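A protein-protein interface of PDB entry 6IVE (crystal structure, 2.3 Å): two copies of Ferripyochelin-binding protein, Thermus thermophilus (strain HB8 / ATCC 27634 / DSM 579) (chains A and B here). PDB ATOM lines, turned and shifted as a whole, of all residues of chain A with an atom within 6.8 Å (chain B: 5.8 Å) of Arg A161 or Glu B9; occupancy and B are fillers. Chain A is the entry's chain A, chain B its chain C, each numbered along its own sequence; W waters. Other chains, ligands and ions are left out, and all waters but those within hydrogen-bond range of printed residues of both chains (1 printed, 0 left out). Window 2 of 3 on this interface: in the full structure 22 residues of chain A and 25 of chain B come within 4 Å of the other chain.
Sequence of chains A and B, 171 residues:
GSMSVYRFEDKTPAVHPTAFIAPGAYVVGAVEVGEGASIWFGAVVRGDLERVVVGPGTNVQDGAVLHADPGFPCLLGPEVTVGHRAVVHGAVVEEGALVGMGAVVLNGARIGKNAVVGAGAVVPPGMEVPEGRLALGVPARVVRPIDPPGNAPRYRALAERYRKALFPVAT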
ATOM      1  N   ARG A 156      25.045 -12.943 -19.102  1.00  0.00           N
ATOM      2  CA  ARG A 156      24.776 -14.180 -18.376  1.00  0.00           C
ATOM      3  C   ARG A 156      23.382 -14.700 -18.698  1.00  0.00           C
ATOM      4  O   ARG A 156      23.198 -15.895 -18.954  1.00  0.00           O
ATOM      5  CB  ARG A 156      24.919 -13.965 -16.869  1.00  0.00           C
ATOM      6  CG  ARG A 156      26.305 -14.212 -16.294  1.00  0.00           C
ATOM      7  CD  ARG A 156      26.228 -14.188 -14.770  1.00  0.00           C
ATOM      8  NE  ARG A 156      27.532 -14.271 -14.116  1.00  0.00           N
ATOM      9  CZ  ARG A 156      28.078 -15.403 -13.682  1.00  0.00           C
ATOM     10  NH1 ARG A 156      27.438 -16.554 -13.844  1.00  0.00           N
ATOM     11  NH2 ARG A 156      29.265 -15.384 -13.091  1.00  0.00           N
ATOM     12  N   ALA A 157      22.387 -13.808 -18.702  1.00  0.00           N
ATOM     13  CA  ALA A 157      21.016 -14.231 -18.970  1.00  0.00           C
ATOM     14  C   ALA A 157      20.809 -14.535 -20.446  1.00  0.00           C
ATOM     15  O   ALA A 157      20.155 -15.525 -20.793  1.00  0.00           O
ATOM     16  CB  ALA A 157      20.032 -13.159 -18.498  1.00  0.00           C
ATOM     17  N   LEU A 158      21.355 -13.696 -21.330  1.00  0.00           N
ATOM     18  CA  LEU A 158      21.219 -13.936 -22.762  1.00  0.00           C
ATOM     19  C   LEU A 158      21.897 -15.237 -23.167  1.00  0.00           C
ATOM     20  O   LEU A 158      21.412 -15.949 -24.054  1.00  0.00           O
ATOM     21  CB  LEU A 158      21.795 -12.759 -23.551  1.00  0.00           C
ATOM     22  CG  LEU A 158      21.518 -12.705 -25.056  1.00  0.00           C
ATOM     23  CD1 LEU A 158      20.025 -12.607 -25.339  1.00  0.00           C
ATOM     24  CD2 LEU A 158      22.261 -11.535 -25.695  1.00  0.00           C
ATOM     25  N   ALA A 159      23.022 -15.570 -22.523  1.00  0.00           N
ATOM     26  CA  ALA A 159      23.702 -16.826 -22.824  1.00  0.00           C
ATOM     27  C   ALA A 159      22.858 -18.026 -22.417  1.00  0.00           C
ATOM     28  O   ALA A 159      22.775 -19.011 -23.162  1.00  0.00           O
ATOM     29  CB  ALA A 159      25.063 -16.880 -22.131  1.00  0.00           C
ATOM     30  N   GLU A 160      22.233 -17.970 -21.239  1.00  0.00           N
ATOM     31  CA  GLU A 160      21.410 -19.090 -20.794  1.00  0.00           C
ATOM     32  C   GLU A 160      20.215 -19.300 -21.719  1.00  0.00           C
ATOM     33  O   GLU A 160      19.816 -20.440 -21.979  1.00  0.00           O
ATOM     34  CB  GLU A 160      20.940 -18.869 -19.355  1.00  0.00           C
ATOM     35  CG  GLU A 160      20.335 -20.116 -18.722  1.00  0.00           C
ATOM     36  CD  GLU A 160      19.551 -19.815 -17.459  1.00  0.00           C
ATOM     37  OE1 GLU A 160      20.110 -19.166 -16.548  1.00  0.00           O
ATOM     38  OE2 GLU A 160      18.373 -20.230 -17.378  1.00  0.00           O
ATOM     39  N   ARG A 161      19.634 -18.209 -22.225  1.00  0.00           N
ATOM     40  CA  ARG A 161      18.564 -18.334 -23.211  1.00  0.00           C
ATOM     41  C   ARG A 161      19.072 -18.988 -24.492  1.00  0.00           C
ATOM     42  O   ARG A 161      18.380 -19.818 -25.092  1.00  0.00           O
ATOM     43  CB  ARG A 161      17.957 -16.962 -23.509  1.00  0.00           C
ATOM     44  CG  ARG A 161      17.192 -16.353 -22.342  1.00  0.00           C
ATOM     45  CD  ARG A 161      16.917 -14.870 -22.560  1.00  0.00           C
ATOM     46  NE  ARG A 161      16.024 -14.620 -23.690  1.00  0.00           N
ATOM     47  CZ  ARG A 161      15.660 -13.409 -24.100  1.00  0.00           C
ATOM     48  NH1 ARG A 161      16.115 -12.332 -23.476  1.00  0.00           N
ATOM     49  NH2 ARG A 161      14.842 -13.272 -25.137  1.00  0.00           N
ATOM     50  N   TYR A 162      20.285 -18.627 -24.924  1.00  0.00           N
ATOM     51  CA  TYR A 162      20.858 -19.248 -26.113  1.00  0.00           C
ATOM     52  C   TYR A 162      21.169 -20.720 -25.875  1.00  0.00           C
ATOM     53  O   TYR A 162      21.023 -21.545 -26.783  1.00  0.00           O
ATOM     54  CB  TYR A 162      22.116 -18.499 -26.550  1.00  0.00           C
ATOM     55  CG  TYR A 162      21.858 -17.434 -27.589  1.00  0.00           C
ATOM     56  CD1 TYR A 162      21.536 -16.136 -27.216  1.00  0.00           C
ATOM     57  CD2 TYR A 162      21.937 -17.726 -28.945  1.00  0.00           C
ATOM     58  CE1 TYR A 162      21.298 -15.159 -28.165  1.00  0.00           C
ATOM     59  CE2 TYR A 162      21.703 -16.755 -29.899  1.00  0.00           C
ATOM     60  CZ  TYR A 162      21.383 -15.473 -29.503  1.00  0.00           C
ATOM     61  OH  TYR A 162      21.146 -14.501 -30.449  1.00  0.00           O
ATOM     62  N   ARG A 163      21.596 -21.070 -24.660  1.00  0.00           N
ATOM     63  CA  ARG A 163      21.838 -22.474 -24.353  1.00  0.00           C
ATOM     64  C   ARG A 163      20.548 -23.281 -24.377  1.00  0.00           C
ATOM     65  O   ARG A 163      20.582 -24.491 -24.627  1.00  0.00           O
ATOM     66  CB  ARG A 163      22.533 -22.601 -22.999  1.00  0.00           C
ATOM     67  CG  ARG A 163      23.906 -21.957 -22.973  1.00  0.00           C
ATOM     68  CD  ARG A 163      24.529 -21.967 -21.590  1.00  0.00           C
ATOM     69  NE  ARG A 163      24.768 -23.323 -21.111  1.00  0.00           N
ATOM     70  CZ  ARG A 163      24.121 -23.880 -20.095  1.00  0.00           C
ATOM     71  NH1 ARG A 163      23.198 -23.192 -19.438  1.00  0.00           N
ATOM     72  NH2 ARG A 163      24.405 -25.122 -19.732  1.00  0.00           N
ATOM     73  N   LYS A 164      19.406 -22.633 -24.143  1.00  0.00           N
ATOM     74  CA  LYS A 164      18.123 -23.324 -24.144  1.00  0.00           C
ATOM     75  C   LYS A 164      17.470 -23.383 -25.519  1.00  0.00           C
ATOM     76  O   LYS A 164      16.745 -24.342 -25.804  1.00  0.00           O
ATOM     77  CB  LYS A 164      17.154 -22.647 -23.168  1.00  0.00           C
ATOM     78  CG  LYS A 164      17.499 -22.820 -21.698  1.00  0.00           C
ATOM     79  CD  LYS A 164      16.464 -22.127 -20.821  1.00  0.00           C
ATOM     80  CE  LYS A 164      16.303 -20.666 -21.220  1.00  0.00           C
ATOM     81  NZ  LYS A 164      15.103 -20.032 -20.606  1.00  0.00           N
ATOM     82  N   ALA A 165      17.698 -22.385 -26.381  1.00  0.00           N
ATOM     83  CA  ALA A 165      16.911 -22.289 -27.607  1.00  0.00           C
ATOM     84  C   ALA A 165      17.745 -21.678 -28.737  1.00  0.00           C
ATOM     85  O   ALA A 165      17.548 -20.544 -29.166  1.00  0.00           O
ATOM     86  CB  ALA A 165      15.631 -21.482 -27.374  1.00  0.00           C
ATOM     87  N   LEU A 166      18.690 -22.460 -29.254  1.00  0.00           N
ATOM     88  CA  LEU A 166      19.440 -22.102 -30.453  1.00  0.00           C
ATOM     89  C   LEU A 166      19.412 -23.292 -31.400  1.00  0.00           C
ATOM     90  O   LEU A 166      19.909 -24.370 -31.058  1.00  0.00           O
ATOM     91  CB  LEU A 166      20.882 -21.708 -30.122  1.00  0.00           C
ATOM     92  CG  LEU A 166      21.729 -21.263 -31.318  1.00  0.00           C
ATOM     93  CD1 LEU A 166      21.112 -20.049 -31.998  1.00  0.00           C
ATOM     94  CD2 LEU A 166      23.156 -20.964 -30.889  1.00  0.00           C
ATOM     95  N   PHE A 167      18.831 -23.098 -32.584  1.00  0.00           N
ATOM     96  CA  PHE A 167      18.638 -24.182 -33.536  1.00  0.00           C
ATOM     97  C   PHE A 167      19.091 -23.728 -34.918  1.00  0.00           C
ATOM     98  O   PHE A 167      18.644 -22.673 -35.402  1.00  0.00           O
ATOM     99  CB  PHE A 167      17.165 -24.621 -33.578  1.00  0.00           C
ATOM    100  CG  PHE A 167      16.519 -24.723 -32.221  1.00  0.00           C
ATOM    101  CD1 PHE A 167      16.570 -25.906 -31.501  1.00  0.00           C
ATOM    102  CD2 PHE A 167      15.860 -23.636 -31.669  1.00  0.00           C
ATOM    103  CE1 PHE A 167      15.976 -26.003 -30.254  1.00  0.00           C
ATOM    104  CE2 PHE A 167      15.261 -23.726 -30.423  1.00  0.00           C
ATOM    105  CZ  PHE A 167      15.320 -24.910 -29.714  1.00  0.00           C
ATOM    106  N   ARG B   7      17.982 -19.943 -35.447  1.00  0.00           N
ATOM    107  CA  ARG B   7      16.752 -19.559 -34.767  1.00  0.00           C
ATOM    108  C   ARG B   7      17.027 -19.424 -33.273  1.00  0.00           C
ATOM    109  O   ARG B   7      17.456 -20.386 -32.627  1.00  0.00           O
ATOM    110  CB  ARG B   7      15.662 -20.600 -35.033  1.00  0.00           C
ATOM    111  CG  ARG B   7      14.503 -20.601 -34.041  1.00  0.00           C
ATOM    112  CD  ARG B   7      13.434 -21.621 -34.433  1.00  0.00           C
ATOM    113  NE  ARG B   7      13.451 -22.824 -33.603  1.00  0.00           N
ATOM    114  CZ  ARG B   7      13.587 -24.061 -34.076  1.00  0.00           C
ATOM    115  NH1 ARG B   7      13.726 -24.269 -35.379  1.00  0.00           N
ATOM    116  NH2 ARG B   7      13.581 -25.094 -33.243  1.00  0.00           N
ATOM    117  N   PHE B   8      16.802 -18.229 -32.734  1.00  0.00           N
ATOM    118  CA  PHE B   8      16.907 -17.974 -31.303  1.00  0.00           C
ATOM    119  C   PHE B   8      15.498 -17.906 -30.730  1.00  0.00           C
ATOM    120  O   PHE B   8      14.690 -17.079 -31.169  1.00  0.00           O
ATOM    121  CB  PHE B   8      17.677 -16.680 -31.025  1.00  0.00           C
ATOM    122  CG  PHE B   8      17.628 -16.237 -29.586  1.00  0.00           C
ATOM    123  CD1 PHE B   8      18.216 -17.001 -28.590  1.00  0.00           C
ATOM    124  CD2 PHE B   8      17.008 -15.050 -29.230  1.00  0.00           C
ATOM    125  CE1 PHE B   8      18.175 -16.597 -27.265  1.00  0.00           C
ATOM    126  CE2 PHE B   8      16.966 -14.642 -27.908  1.00  0.00           C
ATOM    127  CZ  PHE B   8      17.553 -15.418 -26.925  1.00  0.00           C
ATOM    128  N   GLU B   9      15.208 -18.774 -29.759  1.00  0.00           N
ATOM    129  CA  GLU B   9      13.865 -18.904 -29.204  1.00  0.00           C
ATOM    130  C   GLU B   9      12.856 -19.090 -30.332  1.00  0.00           C
ATOM    131  O   GLU B   9      12.866 -20.125 -31.006  1.00  0.00           O
ATOM    132  CB  GLU B   9      13.527 -17.697 -28.320  1.00  0.00           C
ATOM    133  CG  GLU B   9      13.891 -17.909 -26.852  1.00  0.00           C
ATOM    134  CD  GLU B   9      14.215 -16.620 -26.110  1.00  0.00           C
ATOM    135  OE1 GLU B   9      14.943 -16.687 -25.097  1.00  0.00           O
ATOM    136  OE2 GLU B   9      13.750 -15.543 -26.535  1.00  0.00           O
ATOM    137  N   ASP B  10      11.997 -18.100 -30.568  1.00  0.00           N
ATOM    138  CA  ASP B  10      11.041 -18.156 -31.667  1.00  0.00           C
ATOM    139  C   ASP B  10      11.387 -17.197 -32.796  1.00  0.00           C
ATOM    140  O   ASP B  10      10.542 -16.943 -33.661  1.00  0.00           O
ATOM    141  CB  ASP B  10       9.625 -17.876 -31.159  1.00  0.00           C
ATOM    142  CG  ASP B  10       9.085 -19.003 -30.306  1.00  0.00           C
ATOM    143  OD1 ASP B  10       9.588 -20.138 -30.443  1.00  0.00           O
ATOM    144  OD2 ASP B  10       8.160 -18.757 -29.503  1.00  0.00           O
ATOM    145  N   LYS B  11      12.604 -16.661 -32.817  1.00  0.00           N
ATOM    146  CA  LYS B  11      13.018 -15.707 -33.838  1.00  0.00           C
ATOM    147  C   LYS B  11      13.890 -16.425 -34.861  1.00  0.00           C
ATOM    148  O   LYS B  11      15.042 -16.770 -34.576  1.00  0.00           O
ATOM    149  CB  LYS B  11      13.755 -14.519 -33.220  1.00  0.00           C
ATOM    150  CG  LYS B  11      12.983 -13.791 -32.117  1.00  0.00           C
ATOM    151  CD  LYS B  11      11.495 -13.649 -32.437  1.00  0.00           C
ATOM    152  CE  LYS B  11      11.233 -12.721 -33.618  1.00  0.00           C
ATOM    153  NZ  LYS B  11       9.985 -13.109 -34.340  1.00  0.00           N
ATOM    154  N   ASP B  48      18.650 -10.264 -30.950  1.00  0.00           N
ATOM    155  CA  ASP B  48      18.007 -10.978 -29.855  1.00  0.00           C
ATOM    156  C   ASP B  48      17.380 -10.001 -28.867  1.00  0.00           C
ATOM    157  O   ASP B  48      16.169 -10.043 -28.634  1.00  0.00           O
ATOM    158  CB  ASP B  48      19.009 -11.910 -29.162  1.00  0.00           C
ATOM    159  CG  ASP B  48      20.395 -11.295 -29.027  1.00  0.00           C
ATOM    160  OD1 ASP B  48      20.506 -10.060 -28.882  1.00  0.00           O
ATOM    161  OD2 ASP B  48      21.382 -12.057 -29.074  1.00  0.00           O
ATOM    162  N   LEU B  49      18.188  -9.111 -28.287  1.00  0.00           N
ATOM    163  CA  LEU B  49      17.642  -8.087 -27.405  1.00  0.00           C
ATOM    164  C   LEU B  49      16.782  -7.079 -28.157  1.00  0.00           C
ATOM    165  O   LEU B  49      15.956  -6.399 -27.538  1.00  0.00           O
ATOM    166  CB  LEU B  49      18.776  -7.357 -26.687  1.00  0.00           C
ATOM    167  CG  LEU B  49      19.799  -8.212 -25.941  1.00  0.00           C
ATOM    168  CD1 LEU B  49      20.983  -7.356 -25.534  1.00  0.00           C
ATOM    169  CD2 LEU B  49      19.173  -8.870 -24.725  1.00  0.00           C
HETATM  170  O   HOH W   1      15.447 -19.121 -24.282  1.00  0.00           O
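Of the 7 printed residues of chain B, 5 touch a printed residue of chain A. Hydrophobic or aromatic side chains of chain B that line the printed part of chain A: Phe B8 and Leu B49. Of the 12 printed residues of chain A, 6 touch a printed residue of chain B. Printed residues of chain A that touch a printed residue of chain B: Leu A158, Arg A161, Tyr A162, Ala A165, Leu A166 and Phe A167. Hydrophobic or aromatic side chains of chain A that line the printed part of chain B: Leu A158, Tyr A162, Ala A165, Leu A166 and Phe A167. Among the printed residues, Asp or Glu carboxylates within 4 Å of a Lys or Arg side-chain nitrogen of the other chain: Arg A161 with Glu B9 (2.7 Å).
Among the printed residues, merely in contact across the chains: Leu A158 with Asp B48 (3.5 Å), Leu A158 with Leu B49 (3.9 Å), Arg A161 with Phe B8 (3.7 Å), Tyr A162 with Phe B8 (3.4 Å), Ala A165 with Phe B8 (3.4 Å) and Leu A166 with Arg B7 (3.4 Å).
O of Ala A165 lies close to O of Arg B7 (3.5 Å). O of Ala A165 lies within hydrogen-bond range of N of Glu B9 (3.0 Å). The guanidinium group (NE) of Arg A161 lies within salt-bridge range of the side-chain carboxylate (OE1) of Glu B9, 2.7 Å away. The backbone NH of Arg B7 lies within hydrogen-bond range of the backbone carbonyl oxygen of Phe A167, 2.8 Å away. The side-chain hydroxyl of Tyr A162 sits at hydrogen-bond distance from the side-chain carboxylate of Asp B48, at 2.8 Å.
Of the printed residues of chain B, Leu A158 touches Asp B48 and Leu B49. Of chain B, only Phe B8 (3.7 Å) and Glu B9 (2.7 Å) come within 4 Å of Arg A161. Printed residues of chain B within 4 Å of Tyr A162: Phe B8 (3.4 Å) and Asp B48 (2.8 Å). Printed residues of chain B within 4 Å of Phe A167: Arg B7. Of chain A, only Arg A161 (2.7 Å) and Ala A165 (3.0 Å) come within 4 Å of Glu B9. Of the printed residues of chain A, Asp B48 touches Leu A158 and Tyr A162. The nearest residue of chain A that does not touch Glu B9 is Phe A167 (4.4 Å).
No position is printed for both chains. Of the 11 pairs that touch across the chains among the printed residues, none has its exchanged pair printed and touching as well.
Water W1 lies within hydrogen-bond range of the side-chain carboxylate of Glu B9 (2.6 Å) and the backbone carbonyl oxygen of Arg A161 (3.1 Å).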
